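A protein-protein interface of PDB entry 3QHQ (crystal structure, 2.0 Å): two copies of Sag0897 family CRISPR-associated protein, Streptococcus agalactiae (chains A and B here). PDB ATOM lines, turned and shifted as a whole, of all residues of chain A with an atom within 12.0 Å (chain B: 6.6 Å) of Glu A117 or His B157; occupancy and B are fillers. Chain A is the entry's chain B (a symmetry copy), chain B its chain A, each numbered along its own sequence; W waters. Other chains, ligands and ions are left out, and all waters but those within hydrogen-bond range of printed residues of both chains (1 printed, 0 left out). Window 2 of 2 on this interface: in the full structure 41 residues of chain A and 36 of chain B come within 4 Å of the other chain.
Printed residues of chain B that touch a printed residue of chain A: Gln B87, Gln B154, His B157 and Tyr B158.
Hydrophobic or aromatic side chains of chain B within 4 Å of the printed part of chain A: His B157 and Tyr B158.
Of the 13 printed residues of chain A, 5 touch a printed residue of chain B.
Hydrophobic or aromatic side chains of chain A that line the printed part of chain B: Leu A118.
Among the printed residues, no Asp or Glu carboxylate lies within 4 Å of a Lys or Arg side-chain nitrogen of the other chain.
OE1 of Gln B87 is in hydrogen-bond range of ND2 of Asn A116 (3.0 Å).
N of Tyr B158 lies close to OE2 of Glu A117 (3.5 Å).
The side-chain amide nitrogen of Gln B87 sits at hydrogen-bond distance from the side-chain carboxylate of Glu A112 (2.8 Å).
N of Asp A119 lies close to NE2 of Gln B154, at 2.9 Å.
Water W1 bridges O of Gln B154 (2.7 Å) and OE2 of Glu A117 (2.9 Å).
Asn A116 touches Tyr B158.
Glu A117 touches His B157.
NE2 of Gln B154 touches CA of Leu A118, at 3.7 Å.
Tyr B158 touches Leu A118 (CD1 to CG, 3.6 Å).
Glu A117 touches two residues of chain B.
His B157 touches one residue of chain A.
Of chain A, only Leu A118 and Asp A119 come within 4 Å of Gln B154.
No residue of chain A comes within 4 Å of Val B155.
No residue of chain A comes within 4 Å of Tyr B156.
Of chain A, only Asn A116 (3.9 Å), Glu A117 (3.2 Å) and Leu A118 (3.6 Å) come within 4 Å of Tyr B158.
No residue of chain A comes within 4 Å of Thr B160.
No residue of chain A comes within 4 Å of Met B189.
No residue of chain A comes within 4 Å of Gln B190.
Of the printed residues of chain B, Asn A116 touches Gln B87 (3.0 Å) and Tyr B158 (3.9 Å).
Of the printed residues of chain A, Gln B87 touches Glu A112 and Asn A116.
Of the printed residues of chain B, Leu A118 touches Gln B154 (3.7 Å) and Tyr B158 (3.6 Å).
Of the printed residues of chain B, Asp A119 touches Gln B154.
Glu A115 touches none of the printed residues of chain B.
Ile A109 touches none of the printed residues of chain B.
The nearest residue of chain A that does not touch His B157 is Leu A118 (6.6 Å).
The nearest printed residue of chain B that does not touch Leu A118 is Val B155 (4.9 Å).
N of Leu A118 lies within hydrogen-bond range of OD1 of Asn A116 (3.0 Å).
ND1 of His B157 is in hydrogen-bond range of O of Met B189 (3.2 Å).
No position is printed for both chains.
Of the 8 pairs that touch across the chains among the printed residues, none has its exchanged pair printed and touching as well.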
ATOM      1  N   ILE A 109     -15.380 -23.380   2.073  1.00  0.00           N
ATOM      2  CA  ILE A 109     -14.681 -23.696   0.822  1.00  0.00           C
ATOM      3  C   ILE A 109     -15.266 -22.867  -0.333  1.00  0.00           C
ATOM      4  O   ILE A 109     -14.526 -22.366  -1.174  1.00  0.00           O
ATOM      5  CB  ILE A 109     -14.719 -25.210   0.497  1.00  0.00           C
ATOM      6  CG1 ILE A 109     -14.024 -26.012   1.605  1.00  0.00           C
ATOM      7  CG2 ILE A 109     -14.048 -25.501  -0.877  1.00  0.00           C
ATOM      8  CD1 ILE A 109     -14.392 -27.499   1.628  1.00  0.00           C
ATOM      9  N   ALA A 110     -16.593 -22.715  -0.350  1.00  0.00           N
ATOM     10  CA  ALA A 110     -17.280 -21.904  -1.366  1.00  0.00           C
ATOM     11  C   ALA A 110     -16.769 -20.470  -1.411  1.00  0.00           C
ATOM     12  O   ALA A 110     -16.576 -19.914  -2.499  1.00  0.00           O
ATOM     13  CB  ALA A 110     -18.795 -21.917  -1.142  1.00  0.00           C
ATOM     14  N   PHE A 111     -16.555 -19.871  -0.240  1.00  0.00           N
ATOM     15  CA  PHE A 111     -15.996 -18.514  -0.168  1.00  0.00           C
ATOM     16  C   PHE A 111     -14.609 -18.452  -0.807  1.00  0.00           C
ATOM     17  O   PHE A 111     -14.314 -17.530  -1.576  1.00  0.00           O
ATOM     18  CB  PHE A 111     -15.927 -18.001   1.274  1.00  0.00           C
ATOM     19  CG  PHE A 111     -15.550 -16.544   1.373  1.00  0.00           C
ATOM     20  CD1 PHE A 111     -14.212 -16.154   1.416  1.00  0.00           C
ATOM     21  CD2 PHE A 111     -16.533 -15.560   1.392  1.00  0.00           C
ATOM     22  CE1 PHE A 111     -13.863 -14.810   1.498  1.00  0.00           C
ATOM     23  CE2 PHE A 111     -16.196 -14.214   1.472  1.00  0.00           C
ATOM     24  CZ  PHE A 111     -14.857 -13.835   1.523  1.00  0.00           C
ATOM     25  N   GLU A 112     -13.760 -19.427  -0.482  1.00  0.00           N
ATOM     26  CA  GLU A 112     -12.428 -19.507  -1.090  1.00  0.00           C
ATOM     27  C   GLU A 112     -12.497 -19.747  -2.605  1.00  0.00           C
ATOM     28  O   GLU A 112     -11.689 -19.203  -3.359  1.00  0.00           O
ATOM     29  CB  GLU A 112     -11.562 -20.570  -0.401  1.00  0.00           C
ATOM     30  CG  GLU A 112     -11.285 -20.291   1.086  1.00  0.00           C
ATOM     31  CD  GLU A 112     -10.758 -18.881   1.350  1.00  0.00           C
ATOM     32  OE1 GLU A 112      -9.908 -18.388   0.574  1.00  0.00           O
ATOM     33  OE2 GLU A 112     -11.198 -18.264   2.342  1.00  0.00           O
ATOM     34  N   CYS A 113     -13.472 -20.541  -3.046  1.00  0.00           N
ATOM     35  CA  CYS A 113     -13.685 -20.747  -4.479  1.00  0.00           C
ATOM     36  C   CYS A 113     -14.031 -19.448  -5.189  1.00  0.00           C
ATOM     37  O   CYS A 113     -13.558 -19.208  -6.293  1.00  0.00           O
ATOM     38  CB  CYS A 113     -14.767 -21.787  -4.733  1.00  0.00           C
ATOM     39  SG  CYS A 113     -14.229 -23.438  -4.389  1.00  0.00           S
ATOM     40  N   LEU A 114     -14.848 -18.615  -4.547  1.00  0.00           N
ATOM     41  CA  LEU A 114     -15.231 -17.328  -5.112  1.00  0.00           C
ATOM     42  C   LEU A 114     -14.058 -16.339  -5.133  1.00  0.00           C
ATOM     43  O   LEU A 114     -13.880 -15.616  -6.118  1.00  0.00           O
ATOM     44  CB  LEU A 114     -16.446 -16.748  -4.377  1.00  0.00           C
ATOM     45  CG  LEU A 114     -17.193 -15.604  -5.078  1.00  0.00           C
ATOM     46  CD1 LEU A 114     -17.655 -15.988  -6.493  1.00  0.00           C
ATOM     47  CD2 LEU A 114     -18.370 -15.131  -4.229  1.00  0.00           C
ATOM     48  N   GLU A 115     -13.251 -16.330  -4.070  1.00  0.00           N
ATOM     49  CA  GLU A 115     -12.040 -15.502  -4.012  1.00  0.00           C
ATOM     50  C   GLU A 115     -11.005 -15.884  -5.073  1.00  0.00           C
ATOM     51  O   GLU A 115     -10.299 -15.020  -5.593  1.00  0.00           O
ATOM     52  CB  GLU A 115     -11.378 -15.569  -2.630  1.00  0.00           C
ATOM     53  CG  GLU A 115     -12.219 -15.034  -1.475  1.00  0.00           C
ATOM     54  CD  GLU A 115     -12.314 -13.527  -1.460  1.00  0.00           C
ATOM     55  OE1 GLU A 115     -11.742 -12.904  -0.539  1.00  0.00           O
ATOM     56  OE2 GLU A 115     -12.958 -12.963  -2.373  1.00  0.00           O
ATOM     57  N   ASN A 116     -10.905 -17.176  -5.372  1.00  0.00           N
ATOM     58  CA  ASN A 116      -9.984 -17.670  -6.399  1.00  0.00           C
ATOM     59  C   ASN A 116     -10.305 -17.059  -7.767  1.00  0.00           C
ATOM     60  O   ASN A 116     -11.474 -16.866  -8.104  1.00  0.00           O
ATOM     61  CB  ASN A 116     -10.049 -19.200  -6.458  1.00  0.00           C
ATOM     62  CG  ASN A 116      -8.929 -19.806  -7.289  1.00  0.00           C
ATOM     63  OD1 ASN A 116      -8.993 -19.827  -8.518  1.00  0.00           O
ATOM     64  ND2 ASN A 116      -7.908 -20.326  -6.617  1.00  0.00           N
ATOM     65  N   GLU A 117      -9.276 -16.754  -8.551  1.00  0.00           N
ATOM     66  CA  GLU A 117      -9.471 -16.067  -9.834  1.00  0.00           C
ATOM     67  C   GLU A 117     -10.302 -16.879 -10.844  1.00  0.00           C
ATOM     68  O   GLU A 117     -10.949 -16.304 -11.723  1.00  0.00           O
ATOM     69  CB  GLU A 117      -8.127 -15.650 -10.448  1.00  0.00           C
ATOM     70  CG  GLU A 117      -7.184 -16.799 -10.794  1.00  0.00           C
ATOM     71  CD  GLU A 117      -5.997 -16.341 -11.628  1.00  0.00           C
ATOM     72  OE1 GLU A 117      -5.197 -15.514 -11.136  1.00  0.00           O
ATOM     73  OE2 GLU A 117      -5.868 -16.806 -12.783  1.00  0.00           O
ATOM     74  N   LEU A 118     -10.281 -18.206 -10.707  1.00  0.00           N
ATOM     75  CA  LEU A 118     -11.012 -19.098 -11.611  1.00  0.00           C
ATOM     76  C   LEU A 118     -12.495 -19.107 -11.296  1.00  0.00           C
ATOM     77  O   LEU A 118     -12.878 -19.009 -10.137  1.00  0.00           O
ATOM     78  CB  LEU A 118     -10.486 -20.529 -11.487  1.00  0.00           C
ATOM     79  CG  LEU A 118      -9.052 -20.790 -11.943  1.00  0.00           C
ATOM     80  CD1 LEU A 118      -8.608 -22.159 -11.454  1.00  0.00           C
ATOM     81  CD2 LEU A 118      -8.942 -20.705 -13.456  1.00  0.00           C
ATOM     82  N   ASP A 119     -13.323 -19.232 -12.327  1.00  0.00           N
ATOM     83  CA  ASP A 119     -14.750 -19.452 -12.145  1.00  0.00           C
ATOM     84  C   ASP A 119     -14.946 -20.914 -11.772  1.00  0.00           C
ATOM     85  O   ASP A 119     -14.881 -21.800 -12.626  1.00  0.00           O
ATOM     86  CB  ASP A 119     -15.532 -19.112 -13.416  1.00  0.00           C
ATOM     87  CG  ASP A 119     -15.594 -17.619 -13.687  1.00  0.00           C
ATOM     88  OD1 ASP A 119     -15.702 -16.832 -12.723  1.00  0.00           O
ATOM     89  OD2 ASP A 119     -15.546 -17.232 -14.871  1.00  0.00           O
ATOM     90  N   LEU A 120     -15.165 -21.158 -10.485  1.00  0.00           N
ATOM     91  CA  LEU A 120     -15.218 -22.521  -9.959  1.00  0.00           C
ATOM     92  C   LEU A 120     -16.634 -22.955  -9.601  1.00  0.00           C
ATOM     93  O   LEU A 120     -17.434 -22.156  -9.111  1.00  0.00           O
ATOM     94  CB  LEU A 120     -14.307 -22.657  -8.733  1.00  0.00           C
ATOM     95  CG  LEU A 120     -12.799 -22.428  -8.934  1.00  0.00           C
ATOM     96  CD1 LEU A 120     -12.090 -22.373  -7.586  1.00  0.00           C
ATOM     97  CD2 LEU A 120     -12.178 -23.508  -9.829  1.00  0.00           C
ATOM     98  N   GLU A 121     -16.930 -24.225  -9.862  1.00  0.00           N
ATOM     99  CA  GLU A 121     -18.174 -24.849  -9.438  1.00  0.00           C
ATOM    100  C   GLU A 121     -17.839 -26.068  -8.575  1.00  0.00           C
ATOM    101  O   GLU A 121     -16.679 -26.461  -8.472  1.00  0.00           O
ATOM    102  CB  GLU A 121     -19.033 -25.242 -10.651  1.00  0.00           C
ATOM    103  CG  GLU A 121     -18.425 -26.326 -11.542  1.00  0.00           C
ATOM    104  CD  GLU A 121     -19.320 -26.721 -12.712  1.00  0.00           C
ATOM    105  OE1 GLU A 121     -19.223 -27.877 -13.167  1.00  0.00           O
ATOM    106  OE2 GLU A 121     -20.117 -25.888 -13.180  1.00  0.00           O
ATOM    107  N   MET B  61       2.022 -22.736 -24.520  1.00  0.00           N
ATOM    108  CA  MET B  61       0.736 -23.417 -24.474  1.00  0.00           C
ATOM    109  C   MET B  61       0.145 -23.374 -25.886  1.00  0.00           C
ATOM    110  O   MET B  61      -0.164 -22.304 -26.412  1.00  0.00           O
ATOM    111  CB  MET B  61      -0.176 -22.724 -23.452  1.00  0.00           C
ATOM    112  CG  MET B  61      -1.530 -23.363 -23.211  1.00  0.00           C
ATOM    113  SD  MET B  61      -2.387 -22.502 -21.871  1.00  0.00           S
ATOM    114  CE  MET B  61      -4.025 -23.208 -22.011  1.00  0.00           C
ATOM    115  N   GLN B  87      -4.915 -21.176   0.417  1.00  0.00           N
ATOM    116  CA  GLN B  87      -5.775 -20.038   0.773  1.00  0.00           C
ATOM    117  C   GLN B  87      -6.274 -20.142   2.224  1.00  0.00           C
ATOM    118  O   GLN B  87      -6.353 -19.133   2.931  1.00  0.00           O
ATOM    119  CB  GLN B  87      -6.948 -19.907  -0.206  1.00  0.00           C
ATOM    120  CG  GLN B  87      -6.560 -19.328  -1.584  1.00  0.00           C
ATOM    121  CD  GLN B  87      -7.732 -19.243  -2.556  1.00  0.00           C
ATOM    122  OE1 GLN B  87      -7.559 -19.407  -3.767  1.00  0.00           O
ATOM    123  NE2 GLN B  87      -8.932 -18.992  -2.031  1.00  0.00           N
ATOM    124  N   ILE B 152     -10.358 -21.593 -22.046  1.00  0.00           N
ATOM    125  CA  ILE B 152      -8.956 -21.887 -22.303  1.00  0.00           C
ATOM    126  C   ILE B 152      -8.086 -20.692 -21.895  1.00  0.00           C
ATOM    127  O   ILE B 152      -7.057 -20.867 -21.247  1.00  0.00           O
ATOM    128  CB  ILE B 152      -8.721 -22.282 -23.791  1.00  0.00           C
ATOM    129  CG1 ILE B 152      -9.368 -23.652 -24.071  1.00  0.00           C
ATOM    130  CG2 ILE B 152      -7.238 -22.301 -24.120  1.00  0.00           C
ATOM    131  CD1 ILE B 152      -9.418 -24.043 -25.547  1.00  0.00           C
ATOM    132  N   ILE B 153      -8.520 -19.483 -22.254  1.00  0.00           N
ATOM    133  CA  ILE B 153      -7.801 -18.258 -21.872  1.00  0.00           C
ATOM    134  C   ILE B 153      -7.766 -18.093 -20.348  1.00  0.00           C
ATOM    135  O   ILE B 153      -6.751 -17.662 -19.786  1.00  0.00           O
ATOM    136  CB  ILE B 153      -8.390 -17.001 -22.580  1.00  0.00           C
ATOM    137  CG1 ILE B 153      -8.163 -17.102 -24.097  1.00  0.00           C
ATOM    138  CG2 ILE B 153      -7.779 -15.706 -22.019  1.00  0.00           C
ATOM    139  CD1 ILE B 153      -9.134 -16.270 -24.931  1.00  0.00           C
ATOM    140  N   GLN B 154      -8.866 -18.446 -19.683  1.00  0.00           N
ATOM    141  CA  GLN B 154      -8.916 -18.419 -18.220  1.00  0.00           C
ATOM    142  C   GLN B 154      -7.864 -19.358 -17.607  1.00  0.00           C
ATOM    143  O   GLN B 154      -7.177 -18.978 -16.661  1.00  0.00           O
ATOM    144  CB  GLN B 154     -10.337 -18.725 -17.695  1.00  0.00           C
ATOM    145  CG  GLN B 154     -10.460 -18.651 -16.173  1.00  0.00           C
ATOM    146  CD  GLN B 154     -11.899 -18.647 -15.649  1.00  0.00           C
ATOM    147  OE1 GLN B 154     -12.614 -17.644 -15.757  1.00  0.00           O
ATOM    148  NE2 GLN B 154     -12.307 -19.749 -15.035  1.00  0.00           N
ATOM    149  N   VAL B 155      -7.737 -20.568 -18.152  1.00  0.00           N
ATOM    150  CA  VAL B 155      -6.718 -21.524 -17.697  1.00  0.00           C
ATOM    151  C   VAL B 155      -5.307 -20.955 -17.916  1.00  0.00           C
ATOM    152  O   VAL B 155      -4.461 -20.997 -17.011  1.00  0.00           O
ATOM    153  CB  VAL B 155      -6.878 -22.915 -18.382  1.00  0.00           C
ATOM    154  CG1 VAL B 155      -5.671 -23.814 -18.109  1.00  0.00           C
ATOM    155  CG2 VAL B 155      -8.163 -23.599 -17.915  1.00  0.00           C
ATOM    156  N   TYR B 156      -5.076 -20.404 -19.108  1.00  0.00           N
ATOM    157  CA  TYR B 156      -3.806 -19.749 -19.436  1.00  0.00           C
ATOM    158  C   TYR B 156      -3.411 -18.672 -18.412  1.00  0.00           C
ATOM    159  O   TYR B 156      -2.268 -18.650 -17.952  1.00  0.00           O
ATOM    160  CB  TYR B 156      -3.862 -19.169 -20.856  1.00  0.00           C
ATOM    161  CG  TYR B 156      -2.649 -18.359 -21.277  1.00  0.00           C
ATOM    162  CD1 TYR B 156      -1.350 -18.847 -21.095  1.00  0.00           C
ATOM    163  CD2 TYR B 156      -2.805 -17.111 -21.882  1.00  0.00           C
ATOM    164  CE1 TYR B 156      -0.242 -18.107 -21.490  1.00  0.00           C
ATOM    165  CE2 TYR B 156      -1.699 -16.365 -22.284  1.00  0.00           C
ATOM    166  CZ  TYR B 156      -0.422 -16.876 -22.087  1.00  0.00           C
ATOM    167  OH  TYR B 156       0.678 -16.145 -22.482  1.00  0.00           O
ATOM    168  N   HIS B 157      -4.349 -17.798 -18.046  1.00  0.00           N
ATOM    169  CA  HIS B 157      -4.067 -16.768 -17.035  1.00  0.00           C
ATOM    170  C   HIS B 157      -3.727 -17.391 -15.681  1.00  0.00           C
ATOM    171  O   HIS B 157      -2.904 -16.862 -14.931  1.00  0.00           O
ATOM    172  CB  HIS B 157      -5.230 -15.781 -16.880  1.00  0.00           C
ATOM    173  CG  HIS B 157      -4.933 -14.652 -15.940  1.00  0.00           C
ATOM    174  ND1 HIS B 157      -4.164 -13.565 -16.299  1.00  0.00           N
ATOM    175  CD2 HIS B 157      -5.288 -14.450 -14.651  1.00  0.00           C
ATOM    176  CE1 HIS B 157      -4.061 -12.741 -15.272  1.00  0.00           C
ATOM    177  NE2 HIS B 157      -4.735 -13.253 -14.259  1.00  0.00           N
ATOM    178  N   TYR B 158      -4.362 -18.522 -15.382  1.00  0.00           N
ATOM    179  CA  TYR B 158      -4.154 -19.211 -14.105  1.00  0.00           C
ATOM    180  C   TYR B 158      -2.764 -19.838 -14.000  1.00  0.00           C
ATOM    181  O   TYR B 158      -2.167 -19.857 -12.925  1.00  0.00           O
ATOM    182  CB  TYR B 158      -5.235 -20.272 -13.892  1.00  0.00           C
ATOM    183  CG  TYR B 158      -5.220 -20.910 -12.515  1.00  0.00           C
ATOM    184  CD1 TYR B 158      -5.525 -20.169 -11.380  1.00  0.00           C
ATOM    185  CD2 TYR B 158      -4.917 -22.265 -12.359  1.00  0.00           C
ATOM    186  CE1 TYR B 158      -5.521 -20.755 -10.108  1.00  0.00           C
ATOM    187  CE2 TYR B 158      -4.910 -22.861 -11.094  1.00  0.00           C
ATOM    188  CZ  TYR B 158      -5.210 -22.102  -9.982  1.00  0.00           C
ATOM    189  OH  TYR B 158      -5.206 -22.694  -8.740  1.00  0.00           O
ATOM    190  N   LEU B 159      -2.261 -20.333 -15.128  1.00  0.00           N
ATOM    191  CA  LEU B 159      -0.985 -21.039 -15.174  1.00  0.00           C
ATOM    192  C   LEU B 159       0.170 -20.056 -15.308  1.00  0.00           C
ATOM    193  O   LEU B 159       0.507 -19.634 -16.414  1.00  0.00           O
ATOM    194  CB  LEU B 159      -0.970 -22.051 -16.330  1.00  0.00           C
ATOM    195  CG  LEU B 159      -1.983 -23.207 -16.291  1.00  0.00           C
ATOM    196  CD1 LEU B 159      -1.914 -24.019 -17.576  1.00  0.00           C
ATOM    197  CD2 LEU B 159      -1.768 -24.104 -15.078  1.00  0.00           C
ATOM    198  N   THR B 160       0.777 -19.707 -14.178  1.00  0.00           N
ATOM    199  CA  THR B 160       1.871 -18.720 -14.139  1.00  0.00           C
ATOM    200  C   THR B 160       3.120 -19.166 -14.906  1.00  0.00           C
ATOM    201  O   THR B 160       3.938 -18.335 -15.310  1.00  0.00           O
ATOM    202  CB  THR B 160       2.282 -18.394 -12.691  1.00  0.00           C
ATOM    203  OG1 THR B 160       2.580 -19.615 -12.004  1.00  0.00           O
ATOM    204  CG2 THR B 160       1.166 -17.655 -11.962  1.00  0.00           C
ATOM    205  N   LEU B 188      -7.771  -7.872 -21.258  1.00  0.00           N
ATOM    206  CA  LEU B 188      -8.067  -7.762 -19.824  1.00  0.00           C
ATOM    207  C   LEU B 188      -7.141  -8.591 -18.934  1.00  0.00           C
ATOM    208  O   LEU B 188      -6.942  -8.251 -17.764  1.00  0.00           O
ATOM    209  CB  LEU B 188      -9.515  -8.181 -19.542  1.00  0.00           C
ATOM    210  CG  LEU B 188     -10.647  -7.167 -19.377  1.00  0.00           C
ATOM    211  CD1 LEU B 188     -10.807  -6.254 -20.583  1.00  0.00           C
ATOM    212  CD2 LEU B 188     -11.952  -7.914 -19.084  1.00  0.00           C
ATOM    213  N   MET B 189      -6.597  -9.679 -19.475  1.00  0.00           N
ATOM    214  CA  MET B 189      -5.769 -10.597 -18.679  1.00  0.00           C
ATOM    215  C   MET B 189      -4.244 -10.461 -18.888  1.00  0.00           C
ATOM    216  O   MET B 189      -3.466 -11.189 -18.263  1.00  0.00           O
ATOM    217  CB  MET B 189      -6.254 -12.053 -18.817  1.00  0.00           C
ATOM    218  CG  MET B 189      -6.478 -12.543 -20.240  1.00  0.00           C
ATOM    219  SD  MET B 189      -4.951 -12.985 -21.093  1.00  0.00           S
ATOM    220  CE  MET B 189      -4.499 -14.442 -20.144  1.00  0.00           C
ATOM    221  N   GLN B 190      -3.843  -9.524 -19.756  1.00  0.00           N
ATOM    222  CA  GLN B 190      -2.450  -9.029 -19.878  1.00  0.00           C
ATOM    223  C   GLN B 190      -1.428  -9.911 -20.607  1.00  0.00           C
ATOM    224  O   GLN B 190      -0.480  -9.389 -21.199  1.00  0.00           O
ATOM    225  CB  GLN B 190      -1.872  -8.598 -18.523  1.00  0.00           C
ATOM    226  CG  GLN B 190      -2.469  -7.316 -17.949  1.00  0.00           C
ATOM    227  CD  GLN B 190      -3.728  -7.563 -17.129  1.00  0.00           C
ATOM    228  OE1 GLN B 190      -3.862  -8.590 -16.455  1.00  0.00           O
ATOM    229  NE2 GLN B 190      -4.653  -6.612 -17.177  1.00  0.00           N
ATOM    230  N   LYS B 191      -1.613 -11.228 -20.562  1.00  0.00           N
ATOM    231  CA  LYS B 191      -0.643 -12.169 -21.138  1.00  0.00           C
ATOM    232  C   LYS B 191      -0.746 -12.274 -22.666  1.00  0.00           C
ATOM    233  O   LYS B 191      -1.798 -12.000 -23.251  1.00  0.00           O
ATOM    234  CB  LYS B 191      -0.790 -13.553 -20.506  1.00  0.00           C
ATOM    235  CG  LYS B 191      -0.721 -13.562 -18.975  1.00  0.00           C
ATOM    236  CD  LYS B 191      -0.975 -14.961 -18.415  1.00  0.00           C
ATOM    237  CE  LYS B 191       0.195 -15.897 -18.651  1.00  0.00           C
ATOM    238  NZ  LYS B 191       0.147 -17.101 -17.760  1.00  0.00           N
HETATM  239  O   HOH W   1      -7.899 -17.200 -14.755  1.00  0.00           O
